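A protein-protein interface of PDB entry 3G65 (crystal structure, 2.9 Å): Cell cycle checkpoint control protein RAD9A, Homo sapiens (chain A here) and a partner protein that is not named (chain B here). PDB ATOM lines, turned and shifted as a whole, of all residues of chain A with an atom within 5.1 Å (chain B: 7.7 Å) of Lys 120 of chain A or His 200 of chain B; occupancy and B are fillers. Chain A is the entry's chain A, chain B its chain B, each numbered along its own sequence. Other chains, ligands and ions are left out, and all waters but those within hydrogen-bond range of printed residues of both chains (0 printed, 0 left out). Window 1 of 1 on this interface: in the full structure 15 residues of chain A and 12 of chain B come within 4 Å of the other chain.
The backbone carbonyl oxygen (O) of Arg 119 of chain A lies within hydrogen-bond range of the backbone NH (N) of Asp 202 of chain B, 3.0 Å away.
The backbone carbonyl oxygen (O) of Thr 121 of chain A lies within hydrogen-bond range of the backbone NH (N) of His 200 of chain B, at 3.0 Å.
The side-chain hydroxyl (OG) of Ser 199 of chain B lies within hydrogen-bond range of a ring nitrogen (ND1) of His 122 of chain A, at 3.1 Å.
The backbone carbonyl oxygen (O) of Ser 198 of chain B sits at hydrogen-bond distance from the backbone NH (N) of Asn 123 of chain A, at 2.8 Å.
The backbone NH (N) of Val 110 of chain A is in hydrogen-bond range of the backbone carbonyl oxygen (O) of His 122 of chain A (2.9 Å).
The guanidinium group (NH1) of Arg 119 of chain A is in hydrogen-bond range of the backbone carbonyl oxygen (O) of Cys 114 of chain A.
The guanidinium group (NE) of Arg 189 of chain B is in salt-bridge range of the side-chain carboxylate (OD1) of Asp 202 of chain B, at 2.8 Å.
The backbone carbonyl oxygen of Leu 190 of chain B sits at hydrogen-bond distance from the backbone NH of Leu 201 of chain B, 2.7 Å away.
OG of Ser 191 of chain B is in hydrogen-bond range of ND1 of His 200 of chain B, at 2.8 Å.
The backbone carbonyl oxygen (O) of Ser 199 of chain B is in hydrogen-bond range of the backbone NH (N) of Thr 192 of chain B (3.0 Å).
Among the printed residues, merely in contact across the chains: Leu 87 of chain A with Glu 169 of chain B, Val 118 of chain A with Leu 201 of chain B, Val 118 of chain A with Asp 202 of chain B, Val 118 of chain A with Tyr 203 of chain B, Arg 119 of chain A with His 200 of chain B, Arg 119 of chain A with Leu 201 of chain B, Lys 120 of chain A with His 200 of chain B, Lys 120 of chain A with Leu 201 of chain B, Thr 121 of chain A with Ser 199 of chain B, His 122 of chain A with Ser 198 of chain B and Asn 123 of chain A with Gly 197 of chain B.
Of the printed residues of chain B, Val 118 of chain A touches Leu 201, Asp 202 and Tyr 203.
Lys 120 of chain A touches just these residues of chain B: His 200 and Leu 201.
Of the printed residues of chain A, Gly 197 of chain B touches Asn 123 (3.4 Å).
Printed residues of chain A within 4 Å of Ser 199 of chain B: Thr 121 and His 122.
Of the printed residues of chain A, His 200 of chain B touches Arg 119 (3.6 Å), Lys 120 (3.4 Å) and Thr 121 (3.0 Å).
The nearest residue of chain A that does not touch His 200 of chain B is Asn 123 of chain A (4.1 Å).
Of the 11 printed residues of chain A, 7 touch a printed residue of chain B.
Printed residues of chain A that touch a printed residue of chain B: Leu 87, Val 118, Arg 119, Lys 120, Thr 121, His 122 and Asn 123.
Hydrophobic or aromatic side chains of chain A within 4 Å of the printed part of chain B: Leu 87, Val 118 and His 122.
Printed residues of chain B that touch a printed residue of chain A: Glu 169, Gly 197, Ser 198, Ser 199, His 200, Leu 201, Asp 202 and Tyr 203.
Hydrophobic or aromatic side chains of chain B within 4 Å of the printed part of chain A: Leu 201 and Tyr 203.
Among the printed residues, no Asp or Glu carboxylate lies within 4 Å of a Lys or Arg side-chain nitrogen of the other chain.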
ATOM      1  N   LEU A  87       4.907   5.257  -6.253  1.00  0.00           N
ATOM      2  CA  LEU A  87       5.390   4.062  -6.932  1.00  0.00           C
ATOM      3  C   LEU A  87       5.666   4.341  -8.406  1.00  0.00           C
ATOM      4  O   LEU A  87       6.542   3.723  -9.009  1.00  0.00           O
ATOM      5  CB  LEU A  87       4.385   2.919  -6.787  1.00  0.00           C
ATOM      6  CG  LEU A  87       4.113   2.436  -5.361  1.00  0.00           C
ATOM      7  CD1 LEU A  87       3.051   1.347  -5.354  1.00  0.00           C
ATOM      8  CD2 LEU A  87       5.396   1.945  -4.707  1.00  0.00           C
ATOM      9  N   VAL A 110      -2.909  -4.473 -11.112  1.00  0.00           N
ATOM     10  CA  VAL A 110      -2.154  -3.331 -11.609  1.00  0.00           C
ATOM     11  C   VAL A 110      -0.657  -3.609 -11.528  1.00  0.00           C
ATOM     12  O   VAL A 110      -0.038  -3.435 -10.480  1.00  0.00           O
ATOM     13  CB  VAL A 110      -2.475  -2.051 -10.815  1.00  0.00           C
ATOM     14  CG1 VAL A 110      -1.737  -0.861 -11.407  1.00  0.00           C
ATOM     15  CG2 VAL A 110      -3.971  -1.797 -10.802  1.00  0.00           C
ATOM     16  N   GLN A 111      -0.082  -4.046 -12.642  1.00  0.00           N
ATOM     17  CA  GLN A 111       1.333  -4.390 -12.686  1.00  0.00           C
ATOM     18  C   GLN A 111       2.172  -3.213 -13.173  1.00  0.00           C
ATOM     19  O   GLN A 111       1.816  -2.544 -14.142  1.00  0.00           O
ATOM     20  CB  GLN A 111       1.557  -5.609 -13.584  1.00  0.00           C
ATOM     21  CG  GLN A 111       2.964  -6.175 -13.527  1.00  0.00           C
ATOM     22  CD  GLN A 111       3.104  -7.459 -14.320  1.00  0.00           C
ATOM     23  OE1 GLN A 111       2.209  -7.834 -15.080  1.00  0.00           O
ATOM     24  NE2 GLN A 111       4.231  -8.140 -14.147  1.00  0.00           N
ATOM     25  N   LEU A 112       3.286  -2.964 -12.493  1.00  0.00           N
ATOM     26  CA  LEU A 112       4.167  -1.856 -12.846  1.00  0.00           C
ATOM     27  C   LEU A 112       5.535  -2.355 -13.302  1.00  0.00           C
ATOM     28  O   LEU A 112       6.285  -2.942 -12.522  1.00  0.00           O
ATOM     29  CB  LEU A 112       4.327  -0.899 -11.662  1.00  0.00           C
ATOM     30  CG  LEU A 112       3.047  -0.260 -11.120  1.00  0.00           C
ATOM     31  CD1 LEU A 112       3.350   0.591  -9.897  1.00  0.00           C
ATOM     32  CD2 LEU A 112       2.363   0.569 -12.194  1.00  0.00           C
ATOM     33  N   CYS A 114       8.736  -1.428 -13.653  1.00  0.00           N
ATOM     34  CA  CYS A 114       9.749  -0.446 -13.287  1.00  0.00           C
ATOM     35  C   CYS A 114      11.069  -0.727 -13.994  1.00  0.00           C
ATOM     36  O   CYS A 114      11.157  -1.624 -14.835  1.00  0.00           O
ATOM     37  CB  CYS A 114       9.953  -0.422 -11.772  1.00  0.00           C
ATOM     38  SG  CYS A 114       8.480   0.034 -10.830  1.00  0.00           S
ATOM     39  N   VAL A 118      12.826  -4.669 -12.034  1.00  0.00           N
ATOM     40  CA  VAL A 118      11.942  -4.752 -10.876  1.00  0.00           C
ATOM     41  C   VAL A 118      10.476  -4.568 -11.266  1.00  0.00           C
ATOM     42  O   VAL A 118      10.113  -3.579 -11.903  1.00  0.00           O
ATOM     43  CB  VAL A 118      12.313  -3.697  -9.815  1.00  0.00           C
ATOM     44  CG1 VAL A 118      11.278  -3.677  -8.700  1.00  0.00           C
ATOM     45  CG2 VAL A 118      13.710  -3.965  -9.261  1.00  0.00           C
ATOM     46  N   ARG A 119       9.636  -5.524 -10.878  1.00  0.00           N
ATOM     47  CA  ARG A 119       8.214  -5.471 -11.203  1.00  0.00           C
ATOM     48  C   ARG A 119       7.361  -5.337  -9.944  1.00  0.00           C
ATOM     49  O   ARG A 119       7.630  -5.979  -8.927  1.00  0.00           O
ATOM     50  CB  ARG A 119       7.798  -6.717 -11.988  1.00  0.00           C
ATOM     51  CG  ARG A 119       8.560  -6.922 -13.288  1.00  0.00           C
ATOM     52  CD  ARG A 119       8.231  -5.836 -14.300  1.00  0.00           C
ATOM     53  NE  ARG A 119       8.933  -6.035 -15.565  1.00  0.00           N
ATOM     54  CZ  ARG A 119      10.049  -5.402 -15.911  1.00  0.00           C
ATOM     55  NH1 ARG A 119      10.597  -4.518 -15.087  1.00  0.00           N
ATOM     56  NH2 ARG A 119      10.619  -5.647 -17.084  1.00  0.00           N
ATOM     57  N   LYS A 120       6.331  -4.498 -10.019  1.00  0.00           N
ATOM     58  CA  LYS A 120       5.427  -4.283  -8.894  1.00  0.00           C
ATOM     59  C   LYS A 120       3.989  -4.631  -9.266  1.00  0.00           C
ATOM     60  O   LYS A 120       3.282  -3.822  -9.866  1.00  0.00           O
ATOM     61  CB  LYS A 120       5.501  -2.833  -8.411  1.00  0.00           C
ATOM     62  CG  LYS A 120       6.885  -2.388  -7.976  1.00  0.00           C
ATOM     63  CD  LYS A 120       6.850  -0.996  -7.364  1.00  0.00           C
ATOM     64  CE  LYS A 120       8.232  -0.548  -6.914  1.00  0.00           C
ATOM     65  NZ  LYS A 120       8.201   0.795  -6.274  1.00  0.00           N
ATOM     66  N   THR A 121       3.560  -5.835  -8.904  1.00  0.00           N
ATOM     67  CA  THR A 121       2.202  -6.276  -9.190  1.00  0.00           C
ATOM     68  C   THR A 121       1.264  -5.923  -8.041  1.00  0.00           C
ATOM     69  O   THR A 121       1.621  -6.062  -6.872  1.00  0.00           O
ATOM     70  CB  THR A 121       2.145  -7.793  -9.448  1.00  0.00           C
ATOM     71  OG1 THR A 121       3.069  -8.138 -10.487  1.00  0.00           O
ATOM     72  CG2 THR A 121       0.743  -8.213  -9.859  1.00  0.00           C
ATOM     73  N   HIS A 122       0.065  -5.462  -8.380  1.00  0.00           N
ATOM     74  CA  HIS A 122      -0.927  -5.088  -7.378  1.00  0.00           C
ATOM     75  C   HIS A 122      -2.227  -5.867  -7.536  1.00  0.00           C
ATOM     76  O   HIS A 122      -2.931  -5.719  -8.535  1.00  0.00           O
ATOM     77  CB  HIS A 122      -1.213  -3.586  -7.436  1.00  0.00           C
ATOM     78  CG  HIS A 122      -0.139  -2.743  -6.825  1.00  0.00           C
ATOM     79  ND1 HIS A 122      -0.142  -2.384  -5.495  1.00  0.00           N
ATOM     80  CD2 HIS A 122       0.971  -2.184  -7.363  1.00  0.00           C
ATOM     81  CE1 HIS A 122       0.920  -1.641  -5.239  1.00  0.00           C
ATOM     82  NE2 HIS A 122       1.611  -1.505  -6.356  1.00  0.00           N
ATOM     83  N   ASN A 123      -2.536  -6.697  -6.545  1.00  0.00           N
ATOM     84  CA  ASN A 123      -3.792  -7.435  -6.527  1.00  0.00           C
ATOM     85  C   ASN A 123      -4.812  -6.732  -5.641  1.00  0.00           C
ATOM     86  O   ASN A 123      -4.839  -6.934  -4.427  1.00  0.00           O
ATOM     87  CB  ASN A 123      -3.571  -8.866  -6.039  1.00  0.00           C
ATOM     88  CG  ASN A 123      -2.588  -9.633  -6.902  1.00  0.00           C
ATOM     89  OD1 ASN A 123      -1.902  -9.057  -7.745  1.00  0.00           O
ATOM     90  ND2 ASN A 123      -2.517 -10.943  -6.694  1.00  0.00           N
ATOM     91  N   GLY B 162      17.878   0.644  -4.622  1.00  0.00           N
ATOM     92  CA  GLY B 162      16.734  -0.076  -5.152  1.00  0.00           C
ATOM     93  C   GLY B 162      15.720  -0.457  -4.093  1.00  0.00           C
ATOM     94  O   GLY B 162      14.522  -0.522  -4.368  1.00  0.00           O
ATOM     95  N   ARG B 164      15.136   1.290  -1.437  1.00  0.00           N
ATOM     96  CA  ARG B 164      14.599   2.505  -0.834  1.00  0.00           C
ATOM     97  C   ARG B 164      13.090   2.597  -1.034  1.00  0.00           C
ATOM     98  O   ARG B 164      12.326   2.603  -0.068  1.00  0.00           O
ATOM     99  CB  ARG B 164      15.292   3.746  -1.399  1.00  0.00           C
ATOM    100  CG  ARG B 164      16.752   3.868  -1.002  1.00  0.00           C
ATOM    101  CD  ARG B 164      17.324   5.218  -1.402  1.00  0.00           C
ATOM    102  NE  ARG B 164      18.716   5.363  -0.989  1.00  0.00           N
ATOM    103  CZ  ARG B 164      19.434   6.469  -1.159  1.00  0.00           C
ATOM    104  NH1 ARG B 164      18.891   7.532  -1.734  1.00  0.00           N
ATOM    105  NH2 ARG B 164      20.695   6.511  -0.753  1.00  0.00           N
ATOM    106  N   GLU B 165      12.664   2.659  -2.292  1.00  0.00           N
ATOM    107  CA  GLU B 165      11.241   2.726  -2.617  1.00  0.00           C
ATOM    108  C   GLU B 165      10.509   1.453  -2.194  1.00  0.00           C
ATOM    109  O   GLU B 165       9.281   1.436  -2.082  1.00  0.00           O
ATOM    110  CB  GLU B 165      11.033   2.983  -4.111  1.00  0.00           C
ATOM    111  CG  GLU B 165      11.296   4.417  -4.540  1.00  0.00           C
ATOM    112  CD  GLU B 165      10.998   4.648  -6.009  1.00  0.00           C
ATOM    113  OE1 GLU B 165      11.123   3.691  -6.801  1.00  0.00           O
ATOM    114  OE2 GLU B 165      10.642   5.787  -6.375  1.00  0.00           O
ATOM    115  N   ALA B 166      11.272   0.391  -1.961  1.00  0.00           N
ATOM    116  CA  ALA B 166      10.702  -0.875  -1.524  1.00  0.00           C
ATOM    117  C   ALA B 166      10.113  -0.754  -0.125  1.00  0.00           C
ATOM    118  O   ALA B 166       8.896  -0.698   0.043  1.00  0.00           O
ATOM    119  CB  ALA B 166      11.755  -1.973  -1.564  1.00  0.00           C
ATOM    120  N   GLU B 169       7.519   2.620   0.701  1.00  0.00           N
ATOM    121  CA  GLU B 169       6.114   2.489   0.322  1.00  0.00           C
ATOM    122  C   GLU B 169       5.586   1.086   0.597  1.00  0.00           C
ATOM    123  O   GLU B 169       4.538   0.691   0.084  1.00  0.00           O
ATOM    124  CB  GLU B 169       5.921   2.843  -1.154  1.00  0.00           C
ATOM    125  CG  GLU B 169       6.312   4.270  -1.508  1.00  0.00           C
ATOM    126  CD  GLU B 169       5.507   5.306  -0.746  1.00  0.00           C
ATOM    127  OE1 GLU B 169       4.386   4.981  -0.302  1.00  0.00           O
ATOM    128  OE2 GLU B 169       5.996   6.446  -0.594  1.00  0.00           O
ATOM    129  N   LEU B 170       6.317   0.338   1.416  1.00  0.00           N
ATOM    130  CA  LEU B 170       5.956  -1.038   1.739  1.00  0.00           C
ATOM    131  C   LEU B 170       4.888  -1.098   2.825  1.00  0.00           C
ATOM    132  O   LEU B 170       3.928  -1.863   2.723  1.00  0.00           O
ATOM    133  CB  LEU B 170       7.189  -1.823   2.189  1.00  0.00           C
ATOM    134  CG  LEU B 170       6.941  -3.268   2.623  1.00  0.00           C
ATOM    135  CD1 LEU B 170       6.567  -4.129   1.423  1.00  0.00           C
ATOM    136  CD2 LEU B 170       8.170  -3.825   3.332  1.00  0.00           C
ATOM    137  N   GLN B 178       6.154 -11.030   3.504  1.00  0.00           N
ATOM    138  CA  GLN B 178       6.624 -12.308   2.984  1.00  0.00           C
ATOM    139  C   GLN B 178       7.850 -12.139   2.093  1.00  0.00           C
ATOM    140  O   GLN B 178       7.795 -11.467   1.062  1.00  0.00           O
ATOM    141  CB  GLN B 178       5.507 -13.025   2.224  1.00  0.00           C
ATOM    142  CG  GLN B 178       5.895 -14.395   1.698  1.00  0.00           C
ATOM    143  CD  GLN B 178       4.712 -15.155   1.131  1.00  0.00           C
ATOM    144  OE1 GLN B 178       3.559 -14.868   1.458  1.00  0.00           O
ATOM    145  NE2 GLN B 178       4.992 -16.133   0.279  1.00  0.00           N
ATOM    146  N   THR B 180      10.513 -14.127  -0.234  1.00  0.00           N
ATOM    147  CA  THR B 180      10.754 -15.379  -0.938  1.00  0.00           C
ATOM    148  C   THR B 180      11.959 -15.297  -1.869  1.00  0.00           C
ATOM    149  O   THR B 180      12.003 -14.467  -2.777  1.00  0.00           O
ATOM    150  CB  THR B 180       9.515 -15.834  -1.733  1.00  0.00           C
ATOM    151  OG1 THR B 180       9.886 -16.880  -2.640  1.00  0.00           O
ATOM    152  CG2 THR B 180       8.929 -14.675  -2.518  1.00  0.00           C
ATOM    153  N   PHE B 188      13.613 -13.121  -6.365  1.00  0.00           N
ATOM    154  CA  PHE B 188      13.578 -12.424  -5.084  1.00  0.00           C
ATOM    155  C   PHE B 188      12.345 -11.531  -4.989  1.00  0.00           C
ATOM    156  O   PHE B 188      12.309 -10.445  -5.568  1.00  0.00           O
ATOM    157  CB  PHE B 188      14.851 -11.601  -4.880  1.00  0.00           C
ATOM    158  CG  PHE B 188      14.857 -10.797  -3.611  1.00  0.00           C
ATOM    159  CD1 PHE B 188      14.932 -11.423  -2.378  1.00  0.00           C
ATOM    160  CD2 PHE B 188      14.793  -9.413  -3.651  1.00  0.00           C
ATOM    161  CE1 PHE B 188      14.937 -10.685  -1.208  1.00  0.00           C
ATOM    162  CE2 PHE B 188      14.798  -8.671  -2.487  1.00  0.00           C
ATOM    163  CZ  PHE B 188      14.870  -9.308  -1.264  1.00  0.00           C
ATOM    164  N   ARG B 189      11.337 -11.993  -4.256  1.00  0.00           N
ATOM    165  CA  ARG B 189      10.065 -11.284  -4.182  1.00  0.00           C
ATOM    166  C   ARG B 189       9.672 -10.887  -2.762  1.00  0.00           C
ATOM    167  O   ARG B 189       9.670 -11.714  -1.851  1.00  0.00           O
ATOM    168  CB  ARG B 189       8.951 -12.125  -4.814  1.00  0.00           C
ATOM    169  CG  ARG B 189       7.551 -11.598  -4.541  1.00  0.00           C
ATOM    170  CD  ARG B 189       6.487 -12.534  -5.087  1.00  0.00           C
ATOM    171  NE  ARG B 189       6.567 -12.669  -6.538  1.00  0.00           N
ATOM    172  CZ  ARG B 189       5.729 -13.397  -7.269  1.00  0.00           C
ATOM    173  NH1 ARG B 189       4.742 -14.060  -6.683  1.00  0.00           N
ATOM    174  NH2 ARG B 189       5.877 -13.460  -8.585  1.00  0.00           N
ATOM    175  N   LEU B 190       9.339  -9.613  -2.586  1.00  0.00           N
ATOM    176  CA  LEU B 190       8.798  -9.120  -1.323  1.00  0.00           C
ATOM    177  C   LEU B 190       7.290  -8.936  -1.471  1.00  0.00           C
ATOM    178  O   LEU B 190       6.825  -8.320  -2.430  1.00  0.00           O
ATOM    179  CB  LEU B 190       9.458  -7.796  -0.939  1.00  0.00           C
ATOM    180  CG  LEU B 190      10.988  -7.803  -0.867  1.00  0.00           C
ATOM    181  CD1 LEU B 190      11.526  -6.390  -0.704  1.00  0.00           C
ATOM    182  CD2 LEU B 190      11.479  -8.700   0.263  1.00  0.00           C
ATOM    183  N   SER B 191       6.526  -9.472  -0.525  1.00  0.00           N
ATOM    184  CA  SER B 191       5.071  -9.458  -0.640  1.00  0.00           C
ATOM    185  C   SER B 191       4.372  -9.010   0.639  1.00  0.00           C
ATOM    186  O   SER B 191       4.874  -9.222   1.742  1.00  0.00           O
ATOM    187  CB  SER B 191       4.563 -10.840  -1.058  1.00  0.00           C
ATOM    188  OG  SER B 191       5.229 -11.294  -2.225  1.00  0.00           O
ATOM    189  N   THR B 192       3.209  -8.387   0.477  1.00  0.00           N
ATOM    190  CA  THR B 192       2.393  -7.959   1.607  1.00  0.00           C
ATOM    191  C   THR B 192       0.932  -8.313   1.359  1.00  0.00           C
ATOM    192  O   THR B 192       0.511  -8.477   0.212  1.00  0.00           O
ATOM    193  CB  THR B 192       2.512  -6.443   1.858  1.00  0.00           C
ATOM    194  OG1 THR B 192       2.322  -5.733   0.627  1.00  0.00           O
ATOM    195  CG2 THR B 192       3.879  -6.102   2.431  1.00  0.00           C
ATOM    196  N   PHE B 193       0.161  -8.432   2.436  1.00  0.00           N
ATOM    197  CA  PHE B 193      -1.241  -8.822   2.336  1.00  0.00           C
ATOM    198  C   PHE B 193      -2.100  -8.078   3.350  1.00  0.00           C
ATOM    199  O   PHE B 193      -2.298  -8.544   4.473  1.00  0.00           O
ATOM    200  CB  PHE B 193      -1.390 -10.333   2.535  1.00  0.00           C
ATOM    201  CG  PHE B 193      -0.443 -11.148   1.702  1.00  0.00           C
ATOM    202  CD1 PHE B 193      -0.775 -11.512   0.408  1.00  0.00           C
ATOM    203  CD2 PHE B 193       0.782 -11.545   2.211  1.00  0.00           C
ATOM    204  CE1 PHE B 193       0.098 -12.259  -0.363  1.00  0.00           C
ATOM    205  CE2 PHE B 193       1.657 -12.292   1.447  1.00  0.00           C
ATOM    206  CZ  PHE B 193       1.315 -12.649   0.158  1.00  0.00           C
ATOM    207  N   GLY B 197      -5.262  -5.428  -0.373  1.00  0.00           N
ATOM    208  CA  GLY B 197      -5.078  -6.673  -1.095  1.00  0.00           C
ATOM    209  C   GLY B 197      -3.679  -7.231  -0.921  1.00  0.00           C
ATOM    210  O   GLY B 197      -3.165  -7.306   0.194  1.00  0.00           O
ATOM    211  N   SER B 198      -3.063  -7.621  -2.032  1.00  0.00           N
ATOM    212  CA  SER B 198      -1.715  -8.177  -2.001  1.00  0.00           C
ATOM    213  C   SER B 198      -0.807  -7.511  -3.029  1.00  0.00           C
ATOM    214  O   SER B 198      -1.116  -7.485  -4.218  1.00  0.00           O
ATOM    215  CB  SER B 198      -1.752  -9.689  -2.232  1.00  0.00           C
ATOM    216  OG  SER B 198      -2.274 -10.004  -3.511  1.00  0.00           O
ATOM    217  N   SER B 199       0.315  -6.973  -2.562  1.00  0.00           N
ATOM    218  CA  SER B 199       1.274  -6.322  -3.446  1.00  0.00           C
ATOM    219  C   SER B 199       2.606  -7.066  -3.442  1.00  0.00           C
ATOM    220  O   SER B 199       3.162  -7.357  -2.382  1.00  0.00           O
ATOM    221  CB  SER B 199       1.481  -4.865  -3.032  1.00  0.00           C
ATOM    222  OG  SER B 199       0.254  -4.154  -3.042  1.00  0.00           O
ATOM    223  N   HIS B 200       3.113  -7.372  -4.631  1.00  0.00           N
ATOM    224  CA  HIS B 200       4.358  -8.120  -4.757  1.00  0.00           C
ATOM    225  C   HIS B 200       5.445  -7.295  -5.439  1.00  0.00           C
ATOM    226  O   HIS B 200       5.170  -6.526  -6.360  1.00  0.00           O
ATOM    227  CB  HIS B 200       4.122  -9.424  -5.524  1.00  0.00           C
ATOM    228  CG  HIS B 200       2.965 -10.225  -5.013  1.00  0.00           C
ATOM    229  ND1 HIS B 200       3.095 -11.174  -4.022  1.00  0.00           N
ATOM    230  CD2 HIS B 200       1.654 -10.216  -5.354  1.00  0.00           C
ATOM    231  CE1 HIS B 200       1.916 -11.716  -3.775  1.00  0.00           C
ATOM    232  NE2 HIS B 200       1.024 -11.152  -4.570  1.00  0.00           N
ATOM    233  N   LEU B 201       6.681  -7.467  -4.981  1.00  0.00           N
ATOM    234  CA  LEU B 201       7.822  -6.743  -5.527  1.00  0.00           C
ATOM    235  C   LEU B 201       8.924  -7.720  -5.924  1.00  0.00           C
ATOM    236  O   LEU B 201       9.555  -8.334  -5.065  1.00  0.00           O
ATOM    237  CB  LEU B 201       8.356  -5.747  -4.496  1.00  0.00           C
ATOM    238  CG  LEU B 201       9.578  -4.918  -4.892  1.00  0.00           C
ATOM    239  CD1 LEU B 201       9.209  -3.915  -5.967  1.00  0.00           C
ATOM    240  CD2 LEU B 201      10.150  -4.211  -3.678  1.00  0.00           C
ATOM    241  N   ASP B 202       9.156  -7.858  -7.225  1.00  0.00           N
ATOM    242  CA  ASP B 202      10.115  -8.837  -7.726  1.00  0.00           C
ATOM    243  C   ASP B 202      11.473  -8.228  -8.071  1.00  0.00           C
ATOM    244  O   ASP B 202      11.575  -7.045  -8.397  1.00  0.00           O
ATOM    245  CB  ASP B 202       9.545  -9.567  -8.945  1.00  0.00           C
ATOM    246  CG  ASP B 202       8.304 -10.371  -8.615  1.00  0.00           C
ATOM    247  OD1 ASP B 202       7.908 -10.398  -7.430  1.00  0.00           O
ATOM    248  OD2 ASP B 202       7.723 -10.977  -9.539  1.00  0.00           O
ATOM    249  N   TYR B 203      12.510  -9.056  -7.999  1.00  0.00           N
ATOM    250  CA  TYR B 203      13.866  -8.647  -8.346  1.00  0.00           C
ATOM    251  C   TYR B 203      14.526  -9.696  -9.236  1.00  0.00           C
ATOM    252  O   TYR B 203      15.130 -10.648  -8.740  1.00  0.00           O
ATOM    253  CB  TYR B 203      14.704  -8.429  -7.086  1.00  0.00           C
ATOM    254  CG  TYR B 203      14.449  -7.109  -6.400  1.00  0.00           C
ATOM    255  CD1 TYR B 203      15.313  -6.037  -6.574  1.00  0.00           C
ATOM    256  CD2 TYR B 203      13.346  -6.933  -5.576  1.00  0.00           C
ATOM    257  CE1 TYR B 203      15.087  -4.827  -5.949  1.00  0.00           C
ATOM    258  CE2 TYR B 203      13.110  -5.726  -4.947  1.00  0.00           C
ATOM    259  CZ  TYR B 203      13.983  -4.677  -5.137  1.00  0.00           C
ATOM    260  OH  TYR B 203      13.756  -3.472  -4.513  1.00  0.00           O
